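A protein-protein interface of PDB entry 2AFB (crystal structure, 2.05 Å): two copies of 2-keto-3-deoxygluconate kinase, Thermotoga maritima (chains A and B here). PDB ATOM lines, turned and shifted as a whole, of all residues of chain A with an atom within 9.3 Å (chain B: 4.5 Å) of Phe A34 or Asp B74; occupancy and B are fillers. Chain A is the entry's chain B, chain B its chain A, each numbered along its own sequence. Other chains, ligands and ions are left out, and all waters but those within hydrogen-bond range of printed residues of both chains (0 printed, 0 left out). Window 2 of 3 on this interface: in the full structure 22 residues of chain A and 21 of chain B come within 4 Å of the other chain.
The side-chain amide oxygen of Asn B70 lies within hydrogen-bond range of the backbone NH of Leu B72, 2.9 Å away. The side-chain carboxylate (OD1) of Asp B74 lies within salt-bridge range of the guanidinium group (NH2) of Arg B92 (3.0 Å). The side-chain carboxylate (OE2) of Glu A103 lies within hydrogen-bond range of the backbone NH (N) of Ile A33 (2.9 Å). O of Phe A101 lies within hydrogen-bond range of N of Val A114, at 2.9 Å. O of Lys A112 lies within hydrogen-bond range of N of Glu A103.
CG2 of Ile A33 touches CB of Pro B71, at 3.5 Å. CD2 of Leu B72 touches CG2 of Ile A33, 3.9 Å away. Phe A34 touches Asp B74 (CE1 to O, 3.5 Å). Ala B75 touches Phe A34. CD1 of Leu B72 touches CE1 of Phe A101, at 3.4 Å. Lys A112 touches Pro B71 (CE to CG, 3.9 Å). CG2 of Val A114 touches CD of Pro B71 (3.8 Å).
Of the printed residues of chain B, Ile A33 touches Pro B71 (3.5 Å) and Leu B72 (3.9 Å). Of chain B, only Asp B74 (3.5 Å) and Ala B75 (3.8 Å) come within 4 Å of Phe A34. Asp A37 touches none of the printed residues of chain B. Printed residues of chain B within 4 Å of Phe A101: Leu B72 (3.4 Å). Arg A109 touches none of the printed residues of chain B. Of the printed residues of chain B, Lys A112 touches Pro B71. Printed residues of chain B within 4 Å of Val A114: Pro B71. Of chain A, only Ile A33, Lys A112 and Val A114 come within 4 Å of Pro B71. Printed residues of chain A within 4 Å of Leu B72: Ile A33 and Phe A101. No residue of chain A comes within 4 Å of Gly B73. Of chain A, only Phe A34 (3.5 Å) comes within 4 Å of Asp B74. Of chain A, only Phe A34 comes within 4 Å of Ala B75. No residue of chain A comes within 4 Å of Ala B77. The nearest residue of chain A that does not touch Asp B74 is Ile A33 (7.2 Å).
Printed residues of chain A that touch a printed residue of chain B: Ile A33, Phe A34, Phe A101, Lys A112 and Val A114. Hydrophobic or aromatic side chains of chain A within 4 Å of the printed part of chain B: Ile A33, Phe A34, Phe A101 and Val A114. Along chain A the printed residues that touch a printed residue of chain B span positions 33 to 114. Hydrophobic or aromatic side chains of chain B that line the printed part of chain A: Pro B71 and Leu B72. Among the printed residues, 7 pairs touch across the chains. Among the printed residues, no Asp or Glu carboxylate lies within 4 Å of a Lys or Arg side-chain nitrogen of the other chain.
No position is printed for both chains.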
ATOM      1  N   PRO A  27      31.238 -27.874  20.310  1.00  0.00           N
ATOM      2  CA  PRO A  27      29.843 -27.867  19.915  1.00  0.00           C
ATOM      3  C   PRO A  27      29.618 -26.748  18.904  1.00  0.00           C
ATOM      4  O   PRO A  27      30.308 -25.688  18.957  1.00  0.00           O
ATOM      5  CB  PRO A  27      29.092 -27.521  21.205  1.00  0.00           C
ATOM      6  CG  PRO A  27      30.014 -27.738  22.283  1.00  0.00           C
ATOM      7  CD  PRO A  27      31.374 -27.434  21.705  1.00  0.00           C
ATOM      8  N   HIS A  30      27.418 -21.953  19.311  1.00  0.00           N
ATOM      9  CA  HIS A  30      27.593 -21.448  20.679  1.00  0.00           C
ATOM     10  C   HIS A  30      27.005 -22.348  21.776  1.00  0.00           C
ATOM     11  O   HIS A  30      26.839 -21.897  22.895  1.00  0.00           O
ATOM     12  CB  HIS A  30      27.089 -20.005  20.791  1.00  0.00           C
ATOM     13  CG  HIS A  30      27.899 -19.017  19.994  1.00  0.00           C
ATOM     14  ND1 HIS A  30      29.249 -18.802  20.215  1.00  0.00           N
ATOM     15  CD2 HIS A  30      27.558 -18.197  18.967  1.00  0.00           C
ATOM     16  CE1 HIS A  30      29.702 -17.890  19.362  1.00  0.00           C
ATOM     17  NE2 HIS A  30      28.693 -17.499  18.598  1.00  0.00           N
ATOM     18  N   LYS A  31      26.656 -23.590  21.428  1.00  0.00           N
ATOM     19  CA  LYS A  31      26.226 -24.556  22.415  1.00  0.00           C
ATOM     20  C   LYS A  31      27.340 -24.884  23.408  1.00  0.00           C
ATOM     21  O   LYS A  31      28.545 -24.821  23.098  1.00  0.00           O
ATOM     22  CB  LYS A  31      25.719 -25.828  21.766  1.00  0.00           C
ATOM     23  CG  LYS A  31      24.341 -25.686  21.104  1.00  0.00           C
ATOM     24  CD  LYS A  31      23.926 -27.047  20.465  1.00  0.00           C
ATOM     25  CE  LYS A  31      22.446 -27.230  20.215  1.00  0.00           C
ATOM     26  NZ  LYS A  31      22.245 -28.616  19.608  1.00  0.00           N
ATOM     27  N   ARG A  32      26.911 -25.170  24.628  1.00  0.00           N
ATOM     28  CA  ARG A  32      27.764 -25.727  25.673  1.00  0.00           C
ATOM     29  C   ARG A  32      27.840 -27.249  25.552  1.00  0.00           C
ATOM     30  O   ARG A  32      26.905 -27.905  25.063  1.00  0.00           O
ATOM     31  CB  ARG A  32      27.235 -25.314  27.071  1.00  0.00           C
ATOM     32  CG  ARG A  32      27.093 -23.790  27.200  1.00  0.00           C
ATOM     33  CD  ARG A  32      27.259 -23.252  28.559  1.00  0.00           C
ATOM     34  NE  ARG A  32      28.583 -23.533  29.055  1.00  0.00           N
ATOM     35  CZ  ARG A  32      29.021 -23.208  30.265  1.00  0.00           C
ATOM     36  NH1 ARG A  32      28.259 -22.551  31.117  1.00  0.00           N
ATOM     37  NH2 ARG A  32      30.238 -23.536  30.624  1.00  0.00           N
ATOM     38  N   ILE A  33      28.974 -27.800  25.974  1.00  0.00           N
ATOM     39  CA  ILE A  33      29.211 -29.253  25.983  1.00  0.00           C
ATOM     40  C   ILE A  33      28.038 -30.050  26.552  1.00  0.00           C
ATOM     41  O   ILE A  33      27.628 -31.064  25.975  1.00  0.00           O
ATOM     42  CB  ILE A  33      30.487 -29.531  26.798  1.00  0.00           C
ATOM     43  CG1 ILE A  33      31.707 -29.040  25.998  1.00  0.00           C
ATOM     44  CG2 ILE A  33      30.626 -30.997  27.169  1.00  0.00           C
ATOM     45  CD1 ILE A  33      33.023 -28.794  26.837  1.00  0.00           C
ATOM     46  N   PHE A  34      27.497 -29.564  27.675  1.00  0.00           N
ATOM     47  CA  PHE A  34      26.338 -30.149  28.329  1.00  0.00           C
ATOM     48  C   PHE A  34      25.117 -30.311  27.429  1.00  0.00           C
ATOM     49  O   PHE A  34      24.345 -31.247  27.601  1.00  0.00           O
ATOM     50  CB  PHE A  34      25.952 -29.308  29.566  1.00  0.00           C
ATOM     51  CG  PHE A  34      24.827 -29.871  30.381  1.00  0.00           C
ATOM     52  CD1 PHE A  34      24.996 -31.017  31.137  1.00  0.00           C
ATOM     53  CD2 PHE A  34      23.601 -29.258  30.417  1.00  0.00           C
ATOM     54  CE1 PHE A  34      23.954 -31.552  31.879  1.00  0.00           C
ATOM     55  CE2 PHE A  34      22.558 -29.780  31.206  1.00  0.00           C
ATOM     56  CZ  PHE A  34      22.746 -30.923  31.948  1.00  0.00           C
ATOM     57  N   GLN A  35      24.912 -29.383  26.494  1.00  0.00           N
ATOM     58  CA  GLN A  35      23.673 -29.404  25.738  1.00  0.00           C
ATOM     59  C   GLN A  35      23.794 -30.065  24.345  1.00  0.00           C
ATOM     60  O   GLN A  35      22.799 -30.281  23.678  1.00  0.00           O
ATOM     61  CB  GLN A  35      23.005 -28.011  25.699  1.00  0.00           C
ATOM     62  CG  GLN A  35      23.707 -26.951  24.989  1.00  0.00           C
ATOM     63  CD  GLN A  35      23.268 -25.507  25.375  1.00  0.00           C
ATOM     64  OE1 GLN A  35      24.089 -24.631  25.377  1.00  0.00           O
ATOM     65  NE2 GLN A  35      22.004 -25.278  25.615  1.00  0.00           N
ATOM     66  N   THR A  36      24.985 -30.465  23.931  1.00  0.00           N
ATOM     67  CA  THR A  36      25.182 -30.758  22.522  1.00  0.00           C
ATOM     68  C   THR A  36      25.011 -32.259  22.238  1.00  0.00           C
ATOM     69  O   THR A  36      25.390 -33.093  23.075  1.00  0.00           O
ATOM     70  CB  THR A  36      26.532 -30.270  22.005  1.00  0.00           C
ATOM     71  OG1 THR A  36      26.525 -30.296  20.562  1.00  0.00           O
ATOM     72  CG2 THR A  36      27.693 -31.131  22.558  1.00  0.00           C
ATOM     73  N   ASP A  37      24.465 -32.554  21.051  1.00  0.00           N
ATOM     74  CA  ASP A  37      24.447 -33.906  20.518  1.00  0.00           C
ATOM     75  C   ASP A  37      25.404 -34.133  19.400  1.00  0.00           C
ATOM     76  O   ASP A  37      25.363 -35.188  18.768  1.00  0.00           O
ATOM     77  CB  ASP A  37      23.021 -34.356  20.161  1.00  0.00           C
ATOM     78  CG  ASP A  37      22.469 -33.750  18.872  1.00  0.00           C
ATOM     79  OD1 ASP A  37      23.036 -32.784  18.253  1.00  0.00           O
ATOM     80  OD2 ASP A  37      21.391 -34.278  18.484  1.00  0.00           O
ATOM     81  N   SER A  38      26.261 -33.145  19.148  1.00  0.00           N
ATOM     82  CA  SER A  38      27.402 -33.330  18.268  1.00  0.00           C
ATOM     83  C   SER A  38      28.548 -32.378  18.539  1.00  0.00           C
ATOM     84  O   SER A  38      28.379 -31.369  19.186  1.00  0.00           O
ATOM     85  CB  SER A  38      27.005 -33.185  16.811  1.00  0.00           C
ATOM     86  OG  SER A  38      26.888 -31.836  16.496  1.00  0.00           O
ATOM     87  N   PHE A  39      29.713 -32.756  18.034  1.00  0.00           N
ATOM     88  CA  PHE A  39      30.918 -31.931  18.090  1.00  0.00           C
ATOM     89  C   PHE A  39      31.431 -31.785  16.665  1.00  0.00           C
ATOM     90  O   PHE A  39      31.517 -32.777  15.922  1.00  0.00           O
ATOM     91  CB  PHE A  39      32.021 -32.590  18.893  1.00  0.00           C
ATOM     92  CG  PHE A  39      31.795 -32.610  20.336  1.00  0.00           C
ATOM     93  CD1 PHE A  39      31.673 -31.405  21.059  1.00  0.00           C
ATOM     94  CD2 PHE A  39      31.758 -33.816  21.017  1.00  0.00           C
ATOM     95  CE1 PHE A  39      31.456 -31.435  22.441  1.00  0.00           C
ATOM     96  CE2 PHE A  39      31.567 -33.864  22.411  1.00  0.00           C
ATOM     97  CZ  PHE A  39      31.404 -32.672  23.115  1.00  0.00           C
ATOM     98  N   PHE A 101      38.377 -30.106  24.204  1.00  0.00           N
ATOM     99  CA  PHE A 101      36.989 -29.725  23.921  1.00  0.00           C
ATOM    100  C   PHE A 101      36.926 -28.221  24.109  1.00  0.00           C
ATOM    101  O   PHE A 101      37.448 -27.703  25.070  1.00  0.00           O
ATOM    102  CB  PHE A 101      36.023 -30.385  24.901  1.00  0.00           C
ATOM    103  CG  PHE A 101      36.082 -31.892  24.901  1.00  0.00           C
ATOM    104  CD1 PHE A 101      37.033 -32.567  25.649  1.00  0.00           C
ATOM    105  CD2 PHE A 101      35.171 -32.626  24.180  1.00  0.00           C
ATOM    106  CE1 PHE A 101      37.110 -33.947  25.659  1.00  0.00           C
ATOM    107  CE2 PHE A 101      35.225 -34.002  24.160  1.00  0.00           C
ATOM    108  CZ  PHE A 101      36.202 -34.678  24.892  1.00  0.00           C
ATOM    109  N   GLU A 103      34.221 -24.929  24.013  1.00  0.00           N
ATOM    110  CA  GLU A 103      32.987 -24.184  23.922  1.00  0.00           C
ATOM    111  C   GLU A 103      33.418 -22.820  23.457  1.00  0.00           C
ATOM    112  O   GLU A 103      34.226 -22.170  24.116  1.00  0.00           O
ATOM    113  CB  GLU A 103      32.328 -24.029  25.284  1.00  0.00           C
ATOM    114  CG  GLU A 103      31.860 -25.294  25.923  1.00  0.00           C
ATOM    115  CD  GLU A 103      31.211 -25.108  27.318  1.00  0.00           C
ATOM    116  OE1 GLU A 103      31.443 -24.058  28.004  1.00  0.00           O
ATOM    117  OE2 GLU A 103      30.483 -26.059  27.746  1.00  0.00           O
ATOM    118  N   ARG A 109      30.221 -14.453  28.205  1.00  0.00           N
ATOM    119  CA  ARG A 109      30.547 -15.831  28.511  1.00  0.00           C
ATOM    120  C   ARG A 109      31.824 -16.191  27.754  1.00  0.00           C
ATOM    121  O   ARG A 109      31.820 -16.273  26.533  1.00  0.00           O
ATOM    122  CB  ARG A 109      29.409 -16.766  28.167  1.00  0.00           C
ATOM    123  CG  ARG A 109      29.767 -18.233  28.292  1.00  0.00           C
ATOM    124  CD  ARG A 109      28.536 -19.130  28.380  1.00  0.00           C
ATOM    125  NE  ARG A 109      27.865 -19.271  27.086  1.00  0.00           N
ATOM    126  CZ  ARG A 109      28.261 -20.073  26.107  1.00  0.00           C
ATOM    127  NH1 ARG A 109      29.358 -20.836  26.221  1.00  0.00           N
ATOM    128  NH2 ARG A 109      27.557 -20.098  24.997  1.00  0.00           N
ATOM    129  N   LYS A 112      35.620 -21.781  26.711  1.00  0.00           N
ATOM    130  CA  LYS A 112      36.001 -22.699  27.782  1.00  0.00           C
ATOM    131  C   LYS A 112      36.620 -23.914  27.123  1.00  0.00           C
ATOM    132  O   LYS A 112      36.031 -24.496  26.186  1.00  0.00           O
ATOM    133  CB  LYS A 112      34.757 -23.126  28.595  1.00  0.00           C
ATOM    134  CG  LYS A 112      35.064 -23.844  29.906  1.00  0.00           C
ATOM    135  CD  LYS A 112      33.807 -24.447  30.535  1.00  0.00           C
ATOM    136  CE  LYS A 112      34.129 -25.494  31.628  1.00  0.00           C
ATOM    137  NZ  LYS A 112      34.765 -24.829  32.837  1.00  0.00           N
ATOM    138  N   VAL A 114      38.196 -27.772  27.890  1.00  0.00           N
ATOM    139  CA  VAL A 114      38.460 -28.917  28.718  1.00  0.00           C
ATOM    140  C   VAL A 114      39.580 -29.690  28.050  1.00  0.00           C
ATOM    141  O   VAL A 114      39.413 -30.173  26.935  1.00  0.00           O
ATOM    142  CB  VAL A 114      37.225 -29.785  28.781  1.00  0.00           C
ATOM    143  CG1 VAL A 114      37.513 -31.043  29.621  1.00  0.00           C
ATOM    144  CG2 VAL A 114      36.059 -28.960  29.313  1.00  0.00           C
ATOM    145  N   ASN B  70      33.582 -32.361  35.237  1.00  0.00           N
ATOM    146  CA  ASN B  70      33.810 -31.507  34.116  1.00  0.00           C
ATOM    147  C   ASN B  70      32.531 -31.628  33.307  1.00  0.00           C
ATOM    148  O   ASN B  70      31.687 -32.439  33.639  1.00  0.00           O
ATOM    149  CB  ASN B  70      35.144 -31.871  33.398  1.00  0.00           C
ATOM    150  CG  ASN B  70      35.102 -33.206  32.591  1.00  0.00           C
ATOM    151  OD1 ASN B  70      34.047 -33.658  32.201  1.00  0.00           O
ATOM    152  ND2 ASN B  70      36.291 -33.796  32.310  1.00  0.00           N
ATOM    153  N   PRO B  71      32.358 -30.790  32.282  1.00  0.00           N
ATOM    154  CA  PRO B  71      31.134 -30.839  31.501  1.00  0.00           C
ATOM    155  C   PRO B  71      30.805 -32.180  30.860  1.00  0.00           C
ATOM    156  O   PRO B  71      29.637 -32.449  30.630  1.00  0.00           O
ATOM    157  CB  PRO B  71      31.390 -29.818  30.409  1.00  0.00           C
ATOM    158  CG  PRO B  71      32.341 -28.858  30.998  1.00  0.00           C
ATOM    159  CD  PRO B  71      33.246 -29.700  31.814  1.00  0.00           C
ATOM    160  N   LEU B  72      31.795 -33.005  30.537  1.00  0.00           N
ATOM    161  CA  LEU B  72      31.491 -34.321  29.962  1.00  0.00           C
ATOM    162  C   LEU B  72      30.888 -35.251  31.002  1.00  0.00           C
ATOM    163  O   LEU B  72      29.905 -35.926  30.743  1.00  0.00           O
ATOM    164  CB  LEU B  72      32.722 -34.935  29.289  1.00  0.00           C
ATOM    165  CG  LEU B  72      33.071 -34.064  28.057  1.00  0.00           C
ATOM    166  CD1 LEU B  72      34.518 -34.014  27.814  1.00  0.00           C
ATOM    167  CD2 LEU B  72      32.288 -34.473  26.810  1.00  0.00           C
ATOM    168  N   GLY B  73      31.439 -35.248  32.197  1.00  0.00           N
ATOM    169  CA  GLY B  73      30.798 -35.954  33.320  1.00  0.00           C
ATOM    170  C   GLY B  73      29.393 -35.451  33.649  1.00  0.00           C
ATOM    171  O   GLY B  73      28.469 -36.255  33.924  1.00  0.00           O
ATOM    172  N   ASP B  74      29.213 -34.130  33.651  1.00  0.00           N
ATOM    173  CA  ASP B  74      27.855 -33.537  33.840  1.00  0.00           C
ATOM    174  C   ASP B  74      26.847 -34.037  32.723  1.00  0.00           C
ATOM    175  O   ASP B  74      25.681 -34.390  32.983  1.00  0.00           O
ATOM    176  CB  ASP B  74      27.936 -32.022  33.741  1.00  0.00           C
ATOM    177  CG  ASP B  74      28.714 -31.347  34.901  1.00  0.00           C
ATOM    178  OD1 ASP B  74      29.037 -31.995  35.929  1.00  0.00           O
ATOM    179  OD2 ASP B  74      28.982 -30.111  34.774  1.00  0.00           O
ATOM    180  N   ALA B  75      27.305 -34.050  31.481  1.00  0.00           N
ATOM    181  CA  ALA B  75      26.466 -34.440  30.342  1.00  0.00           C
ATOM    182  C   ALA B  75      26.074 -35.922  30.451  1.00  0.00           C
ATOM    183  O   ALA B  75      24.953 -36.287  30.209  1.00  0.00           O
ATOM    184  CB  ALA B  75      27.240 -34.188  29.065  1.00  0.00           C
ATOM    185  N   ALA B  76      27.032 -36.780  30.793  1.00  0.00           N
ATOM    186  CA  ALA B  76      26.773 -38.219  30.956  1.00  0.00           C
ATOM    187  C   ALA B  76      25.712 -38.476  32.012  1.00  0.00           C
ATOM    188  O   ALA B  76      24.765 -39.267  31.809  1.00  0.00           O
ATOM    189  CB  ALA B  76      28.062 -38.948  31.304  1.00  0.00           C
ATOM    190  N   ALA B  77      25.847 -37.761  33.127  1.00  0.00           N
ATOM    191  CA  ALA B  77      24.893 -37.827  34.223  1.00  0.00           C
ATOM    192  C   ALA B  77      23.518 -37.299  33.799  1.00  0.00           C
ATOM    193  O   ALA B  77      22.469 -37.829  34.174  1.00  0.00           O
ATOM    194  CB  ALA B  77      25.409 -37.019  35.385  1.00  0.00           C
ATOM    195  N   GLY B  78      23.517 -36.232  33.024  1.00  0.00           N
ATOM    196  CA  GLY B  78      22.262 -35.669  32.606  1.00  0.00           C
ATOM    197  C   GLY B  78      21.597 -36.562  31.561  1.00  0.00           C
ATOM    198  O   GLY B  78      20.398 -36.661  31.556  1.00  0.00           O
ATOM    199  N   ARG B  92      31.875 -38.471  42.192  1.00  0.00           N
ATOM    200  CA  ARG B  92      32.491 -37.463  41.328  1.00  0.00           C
ATOM    201  C   ARG B  92      33.958 -37.186  41.696  1.00  0.00           C
ATOM    202  O   ARG B  92      34.322 -37.069  42.885  1.00  0.00           O
ATOM    203  CB  ARG B  92      31.677 -36.159  41.356  1.00  0.00           C
ATOM    204  CG  ARG B  92      30.180 -36.315  41.084  1.00  0.00           C
ATOM    205  CD  ARG B  92      29.844 -36.963  39.709  1.00  0.00           C
ATOM    206  NE  ARG B  92      30.341 -36.161  38.613  1.00  0.00           N
ATOM    207  CZ  ARG B  92      29.657 -35.236  37.948  1.00  0.00           C
ATOM    208  NH1 ARG B  92      28.373 -35.016  38.187  1.00  0.00           N
ATOM    209  NH2 ARG B  92      30.265 -34.539  36.985  1.00  0.00           N
